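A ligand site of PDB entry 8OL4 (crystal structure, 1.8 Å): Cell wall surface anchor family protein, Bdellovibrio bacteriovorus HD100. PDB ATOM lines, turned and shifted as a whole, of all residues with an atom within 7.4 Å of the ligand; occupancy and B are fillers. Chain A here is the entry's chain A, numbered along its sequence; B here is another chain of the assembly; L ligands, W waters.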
ATOM      1  N   TYR A 163     -17.451  -2.524 -23.525  1.00  0.00           N
ATOM      2  CA  TYR A 163     -18.923  -2.437 -23.467  1.00  0.00           C
ATOM      3  C   TYR A 163     -19.605  -3.205 -24.594  1.00  0.00           C
ATOM      4  O   TYR A 163     -20.753  -2.885 -24.948  1.00  0.00           O
ATOM      5  CB  TYR A 163     -19.403  -0.979 -23.463  1.00  0.00           C
ATOM      6  CG  TYR A 163     -18.894  -0.198 -22.274  1.00  0.00           C
ATOM      7  CD1 TYR A 163     -19.356  -0.472 -20.977  1.00  0.00           C
ATOM      8  CD2 TYR A 163     -17.937   0.790 -22.433  1.00  0.00           C
ATOM      9  CE1 TYR A 163     -18.886   0.243 -19.884  1.00  0.00           C
ATOM     10  CE2 TYR A 163     -17.453   1.507 -21.343  1.00  0.00           C
ATOM     11  CZ  TYR A 163     -17.920   1.224 -20.079  1.00  0.00           C
ATOM     12  OH  TYR A 163     -17.449   1.936 -19.016  1.00  0.00           O
ATOM     13  N   SER A 208     -14.024  -6.249  -7.749  1.00  0.00           N
ATOM     14  CA  SER A 208     -15.136  -5.434  -8.242  1.00  0.00           C
ATOM     15  C   SER A 208     -15.287  -5.574  -9.757  1.00  0.00           C
ATOM     16  O   SER A 208     -14.312  -5.471 -10.491  1.00  0.00           O
ATOM     17  CB  SER A 208     -14.894  -3.964  -7.883  1.00  0.00           C
ATOM     18  OG  SER A 208     -16.092  -3.225  -7.988  1.00  0.00           O
ATOM     19  N   TYR A 210     -18.179  -4.609 -13.202  1.00  0.00           N
ATOM     20  CA  TYR A 210     -19.416  -4.032 -13.686  1.00  0.00           C
ATOM     21  C   TYR A 210     -19.517  -4.164 -15.200  1.00  0.00           C
ATOM     22  O   TYR A 210     -18.519  -4.354 -15.903  1.00  0.00           O
ATOM     23  CB  TYR A 210     -19.563  -2.556 -13.288  1.00  0.00           C
ATOM     24  CG  TYR A 210     -18.629  -1.546 -13.936  1.00  0.00           C
ATOM     25  CD1 TYR A 210     -17.427  -1.196 -13.325  1.00  0.00           C
ATOM     26  CD2 TYR A 210     -18.971  -0.904 -15.117  1.00  0.00           C
ATOM     27  CE1 TYR A 210     -16.587  -0.259 -13.863  1.00  0.00           C
ATOM     28  CE2 TYR A 210     -18.116   0.074 -15.682  1.00  0.00           C
ATOM     29  CZ  TYR A 210     -16.930   0.383 -15.044  1.00  0.00           C
ATOM     30  OH  TYR A 210     -16.068   1.312 -15.584  1.00  0.00           O
ATOM     31  N   ARG A 219     -20.153   4.109 -24.419  1.00  0.00           N
ATOM     32  CA  ARG A 219     -21.004   4.339 -23.248  1.00  0.00           C
ATOM     33  C   ARG A 219     -21.411   5.809 -23.138  1.00  0.00           C
ATOM     34  O   ARG A 219     -22.573   6.132 -22.846  1.00  0.00           O
ATOM     35  CB  ARG A 219     -20.266   3.887 -21.986  1.00  0.00           C
ATOM     36  CG  ARG A 219     -20.770   4.480 -20.678  1.00  0.00           C
ATOM     37  CD  ARG A 219     -19.903   3.991 -19.494  1.00  0.00           C
ATOM     38  NE  ARG A 219     -20.189   4.788 -18.298  1.00  0.00           N
ATOM     39  CZ  ARG A 219     -19.738   4.519 -17.088  1.00  0.00           C
ATOM     40  NH1 ARG A 219     -18.973   3.444 -16.889  1.00  0.00           N
ATOM     41  NH2 ARG A 219     -20.066   5.304 -16.064  1.00  0.00           N
ATOM     42  N   THR A 220     -20.459   6.719 -23.348  1.00  0.00           N
ATOM     43  CA  THR A 220     -20.716   8.149 -23.191  1.00  0.00           C
ATOM     44  C   THR A 220     -21.809   8.637 -24.130  1.00  0.00           C
ATOM     45  O   THR A 220     -22.563   9.552 -23.775  1.00  0.00           O
ATOM     46  CB  THR A 220     -19.424   8.922 -23.438  1.00  0.00           C
ATOM     47  OG1 THR A 220     -18.403   8.440 -22.549  1.00  0.00           O
ATOM     48  CG2 THR A 220     -19.625  10.420 -23.231  1.00  0.00           C
ATOM     49  N   GLU A 223     -24.716   7.878 -21.879  1.00  0.00           N
ATOM     50  CA  GLU A 223     -24.698   8.352 -20.497  1.00  0.00           C
ATOM     51  C   GLU A 223     -24.722   9.882 -20.396  1.00  0.00           C
ATOM     52  O   GLU A 223     -25.271  10.428 -19.437  1.00  0.00           O
ATOM     53  CB  GLU A 223     -23.465   7.802 -19.771  1.00  0.00           C
ATOM     54  CG  GLU A 223     -23.418   8.112 -18.292  1.00  0.00           C
ATOM     55  CD  GLU A 223     -22.152   7.599 -17.655  1.00  0.00           C
ATOM     56  OE1 GLU A 223     -21.168   7.375 -18.383  1.00  0.00           O
ATOM     57  OE2 GLU A 223     -22.129   7.424 -16.413  1.00  0.00           O
ATOM     58  N   TRP A 230     -29.351   6.566 -17.354  1.00  0.00           N
ATOM     59  CA  TRP A 230     -28.274   5.606 -17.580  1.00  0.00           C
ATOM     60  C   TRP A 230     -27.605   5.352 -16.235  1.00  0.00           C
ATOM     61  O   TRP A 230     -27.194   6.294 -15.567  1.00  0.00           O
ATOM     62  CB  TRP A 230     -27.238   6.116 -18.578  1.00  0.00           C
ATOM     63  CG  TRP A 230     -26.276   5.021 -19.038  1.00  0.00           C
ATOM     64  CD1 TRP A 230     -26.333   4.345 -20.223  1.00  0.00           C
ATOM     65  CD2 TRP A 230     -25.145   4.491 -18.325  1.00  0.00           C
ATOM     66  NE1 TRP A 230     -25.302   3.421 -20.294  1.00  0.00           N
ATOM     67  CE2 TRP A 230     -24.569   3.489 -19.135  1.00  0.00           C
ATOM     68  CE3 TRP A 230     -24.574   4.760 -17.075  1.00  0.00           C
ATOM     69  CZ2 TRP A 230     -23.435   2.757 -18.743  1.00  0.00           C
ATOM     70  CZ3 TRP A 230     -23.430   4.029 -16.671  1.00  0.00           C
ATOM     71  CH2 TRP A 230     -22.886   3.042 -17.511  1.00  0.00           C
ATOM     72  N   HIS A 232     -25.335   2.125 -13.689  1.00  0.00           N
ATOM     73  CA  HIS A 232     -24.764   0.790 -13.542  1.00  0.00           C
ATOM     74  C   HIS A 232     -24.298   0.630 -12.110  1.00  0.00           C
ATOM     75  O   HIS A 232     -23.955   1.615 -11.449  1.00  0.00           O
ATOM     76  CB  HIS A 232     -23.603   0.578 -14.527  1.00  0.00           C
ATOM     77  CG  HIS A 232     -22.254   0.994 -13.996  1.00  0.00           C
ATOM     78  ND1 HIS A 232     -21.536   0.203 -13.134  1.00  0.00           N
ATOM     79  CD2 HIS A 232     -21.500   2.097 -14.214  1.00  0.00           C
ATOM     80  CE1 HIS A 232     -20.388   0.799 -12.838  1.00  0.00           C
ATOM     81  NE2 HIS A 232     -20.345   1.957 -13.481  1.00  0.00           N
ATOM     82  N   SER A 233     -24.300  -0.617 -11.625  1.00  0.00           N
ATOM     83  CA  SER A 233     -23.752  -0.929 -10.310  1.00  0.00           C
ATOM     84  C   SER A 233     -22.501  -1.776 -10.451  1.00  0.00           C
ATOM     85  O   SER A 233     -22.165  -2.290 -11.523  1.00  0.00           O
ATOM     86  CB  SER A 233     -24.773  -1.692  -9.450  1.00  0.00           C
ATOM     87  OG  SER A 233     -24.888  -3.016  -9.951  1.00  0.00           O
ATOM     88  N   HIS A 234     -21.821  -1.942  -9.321  1.00  0.00           N
ATOM     89  CA  HIS A 234     -20.714  -2.873  -9.153  1.00  0.00           C
ATOM     90  C   HIS A 234     -21.163  -4.086  -8.366  1.00  0.00           C
ATOM     91  O   HIS A 234     -22.139  -4.033  -7.609  1.00  0.00           O
ATOM     92  CB  HIS A 234     -19.538  -2.223  -8.416  1.00  0.00           C
ATOM     93  CG  HIS A 234     -18.836  -1.150  -9.170  1.00  0.00           C
ATOM     94  ND1 HIS A 234     -17.535  -1.289  -9.616  1.00  0.00           N
ATOM     95  CD2 HIS A 234     -19.222   0.099  -9.512  1.00  0.00           C
ATOM     96  CE1 HIS A 234     -17.159  -0.177 -10.218  1.00  0.00           C
ATOM     97  NE2 HIS A 234     -18.159   0.688 -10.154  1.00  0.00           N
ATOM     98  N   PRO A 261     -16.212  -2.871 -19.102  1.00  0.00           N
ATOM     99  CA  PRO A 261     -15.552  -1.652 -19.623  1.00  0.00           C
ATOM    100  C   PRO A 261     -14.178  -1.888 -20.218  1.00  0.00           C
ATOM    101  O   PRO A 261     -13.719  -1.050 -20.999  1.00  0.00           O
ATOM    102  CB  PRO A 261     -15.478  -0.750 -18.377  1.00  0.00           C
ATOM    103  CG  PRO A 261     -15.452  -1.714 -17.228  1.00  0.00           C
ATOM    104  CD  PRO A 261     -16.319  -2.877 -17.642  1.00  0.00           C
ATOM    105  N   ARG B 201     -26.101   3.516  -4.705  1.00  0.00           N
ATOM    106  CA  ARG B 201     -24.856   2.803  -4.433  1.00  0.00           C
ATOM    107  C   ARG B 201     -24.485   2.888  -2.963  1.00  0.00           C
ATOM    108  O   ARG B 201     -24.571   3.957  -2.345  1.00  0.00           O
ATOM    109  CB  ARG B 201     -23.715   3.404  -5.243  1.00  0.00           C
ATOM    110  CG  ARG B 201     -23.718   3.106  -6.714  1.00  0.00           C
ATOM    111  CD  ARG B 201     -22.399   3.579  -7.318  1.00  0.00           C
ATOM    112  NE  ARG B 201     -22.330   3.173  -8.716  1.00  0.00           N
ATOM    113  CZ  ARG B 201     -21.230   3.215  -9.465  1.00  0.00           C
ATOM    114  NH1 ARG B 201     -20.076   3.643  -8.946  1.00  0.00           N
ATOM    115  NH2 ARG B 201     -21.298   2.809 -10.718  1.00  0.00           N
ATOM    116  N   SER B 238     -19.122  -2.060  -1.890  1.00  0.00           N
ATOM    117  CA  SER B 238     -18.933  -0.715  -2.417  1.00  0.00           C
ATOM    118  C   SER B 238     -19.361  -0.640  -3.879  1.00  0.00           C
ATOM    119  O   SER B 238     -18.947  -1.455  -4.703  1.00  0.00           O
ATOM    120  CB  SER B 238     -17.470  -0.287  -2.229  1.00  0.00           C
ATOM    121  OG  SER B 238     -17.175   0.864  -2.999  1.00  0.00           O
ATOM    122  N   GLY B 239     -20.218   0.327  -4.190  1.00  0.00           N
ATOM    123  CA  GLY B 239     -20.733   0.442  -5.546  1.00  0.00           C
ATOM    124  C   GLY B 239     -21.912  -0.459  -5.896  1.00  0.00           C
ATOM    125  O   GLY B 239     -22.478  -0.308  -6.986  1.00  0.00           O
ATOM    126  N   VAL B 270     -23.512   6.589  -1.229  1.00  0.00           N
ATOM    127  CA  VAL B 270     -22.810   7.521  -2.102  1.00  0.00           C
ATOM    128  C   VAL B 270     -23.749   8.638  -2.527  1.00  0.00           C
ATOM    129  O   VAL B 270     -24.813   8.397  -3.125  1.00  0.00           O
ATOM    130  CB  VAL B 270     -22.221   6.822  -3.340  1.00  0.00           C
ATOM    131  CG1 VAL B 270     -21.558   7.862  -4.231  1.00  0.00           C
ATOM    132  CG2 VAL B 270     -21.203   5.758  -2.913  1.00  0.00           C
ATOM    133  N   PRO B 274     -23.260  11.902 -10.753  1.00  0.00           N
ATOM    134  CA  PRO B 274     -23.486  10.912 -11.828  1.00  0.00           C
ATOM    135  C   PRO B 274     -24.655   9.992 -11.506  1.00  0.00           C
ATOM    136  O   PRO B 274     -24.824   9.511 -10.382  1.00  0.00           O
ATOM    137  CB  PRO B 274     -22.160  10.152 -11.896  1.00  0.00           C
ATOM    138  CG  PRO B 274     -21.143  11.229 -11.569  1.00  0.00           C
ATOM    139  CD  PRO B 274     -21.818  12.089 -10.489  1.00  0.00           C
ATOM    140  N   TYR B 276     -25.176   7.026 -12.247  1.00  0.00           N
ATOM    141  CA  TYR B 276     -24.880   5.670 -11.799  1.00  0.00           C
ATOM    142  C   TYR B 276     -24.808   5.557 -10.279  1.00  0.00           C
ATOM    143  O   TYR B 276     -24.936   4.450  -9.751  1.00  0.00           O
ATOM    144  CB  TYR B 276     -23.593   5.145 -12.456  1.00  0.00           C
ATOM    145  CG  TYR B 276     -22.343   5.978 -12.311  1.00  0.00           C
ATOM    146  CD1 TYR B 276     -21.756   6.184 -11.064  1.00  0.00           C
ATOM    147  CD2 TYR B 276     -21.714   6.513 -13.436  1.00  0.00           C
ATOM    148  CE1 TYR B 276     -20.556   6.930 -10.947  1.00  0.00           C
ATOM    149  CE2 TYR B 276     -20.544   7.260 -13.321  1.00  0.00           C
ATOM    150  CZ  TYR B 276     -19.966   7.455 -12.093  1.00  0.00           C
ATOM    151  OH  TYR B 276     -18.789   8.176 -12.002  1.00  0.00           O
ATOM    152  N   ASN B 277     -24.611   6.673  -9.575  1.00  0.00           N
ATOM    153  CA  ASN B 277     -24.644   6.631  -8.106  1.00  0.00           C
ATOM    154  C   ASN B 277     -26.047   6.381  -7.569  1.00  0.00           C
ATOM    155  O   ASN B 277     -26.203   5.851  -6.464  1.00  0.00           O
ATOM    156  CB  ASN B 277     -24.086   7.928  -7.520  1.00  0.00           C
ATOM    157  CG  ASN B 277     -22.623   8.107  -7.840  1.00  0.00           C
ATOM    158  OD1 ASN B 277     -21.836   7.212  -7.592  1.00  0.00           O
ATOM    159  ND2 ASN B 277     -22.258   9.232  -8.413  1.00  0.00           N
HETATM  160  C1  LIG L   1     -14.879   4.836 -11.661  1.00  0.00           C
HETATM  161  C2  LIG L   1     -16.064   4.235 -10.916  1.00  0.00           C
HETATM  162  C3  LIG L   1     -16.991   3.612 -11.940  1.00  0.00           C
HETATM  163  C4  LIG L   1     -17.438   4.664 -12.927  1.00  0.00           C
HETATM  164  C5  LIG L   1     -16.226   5.302 -13.584  1.00  0.00           C
HETATM  165  C6  LIG L   1     -16.610   6.464 -14.461  1.00  0.00           C
HETATM  166  C7  LIG L   1     -16.270   3.219  -8.681  1.00  0.00           C
HETATM  167  C8  LIG L   1     -16.096   1.936  -7.923  1.00  0.00           C
HETATM  168  N1  LIG L   1     -15.719   3.258  -9.896  1.00  0.00           N
HETATM  169  O1  LIG L   1     -13.979   5.390 -10.753  1.00  0.00           O
HETATM  170  O2  LIG L   1     -18.132   3.033 -11.342  1.00  0.00           O
HETATM  171  O3  LIG L   1     -18.256   3.990 -13.858  1.00  0.00           O
HETATM  172  O4  LIG L   1     -15.333   5.815 -12.572  1.00  0.00           O
HETATM  173  O5  LIG L   1     -16.876   6.040 -15.791  1.00  0.00           O
HETATM  174  O6  LIG L   1     -16.879   4.168  -8.203  1.00  0.00           O
HETATM  175  O   HOH W   1     -18.999   3.663  -5.906  1.00  0.00           O
HETATM  176  O   HOH W   2     -19.345   6.089  -7.091  1.00  0.00           O
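O2 of the ligand is in hydrogen-bond range of NE2 of His 234 (2.6 Å). A ring nitrogen (NE2) of His 232 sits at hydrogen-bond distance from an oxygen (O3) of the ligand (2.9 Å). An oxygen (O3) of the ligand lies within hydrogen-bond range of the guanidinium group (NH2) of Arg 219 (3.1 Å). The guanidinium group (NH1) of Arg 201 of chain B lies within hydrogen-bond range of an oxygen (O2) of the ligand, at 3.1 Å.
A ring nitrogen (ND1) of His 234 lies within hydrogen-bond range of the side-chain hydroxyl (OG) of Ser 208 (2.9 Å). The backbone NH (N) of His 234 lies within hydrogen-bond range of the backbone carbonyl oxygen (O) of Gly 239 of chain B (2.9 Å). The backbone carbonyl oxygen (O) of His 232 sits at hydrogen-bond distance from the guanidinium group (NH2) of Arg 201 of chain B, at 3.0 Å. The side-chain carboxylate of Glu 223 is in salt-bridge range of the guanidinium group of Arg 219. The side-chain hydroxyl (OH) of Tyr 163 sits at hydrogen-bond distance from the guanidinium group (NH1) of Arg 219. The guanidinium group of Arg 201 of chain B sits at hydrogen-bond distance from the backbone carbonyl oxygen of Tyr 276 of chain B (3.1 Å). The backbone NH (N) of Arg 201 of chain B sits at hydrogen-bond distance from the backbone carbonyl oxygen (O) of Asn 277 of chain B, at 2.9 Å.
Residues that only touch the ligand: Tyr 276 of chain B (3.7 Å) and Tyr 210 (3.9 Å). Hydrophobic or aromatic side chains within 4 Å of the ligand: His 232, His 234 and Tyr 276 of chain B. Within 4 Å of the ligand: Tyr 210, Arg 219, His 232, His 234, Arg 201 of chain B and Tyr 276 of chain B.
Water W1 bridges an oxygen (O6) of the ligand (3.2 Å) and the guanidinium group (NH1) of Arg 201 of chain B (3.2 Å). Water W2 lies within hydrogen-bond range of the side-chain amide oxygen (OD1) of Asn 277 of chain B, the guanidinium group (NH1) of Arg 201 of chain B and an oxygen (O6) of the ligand.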
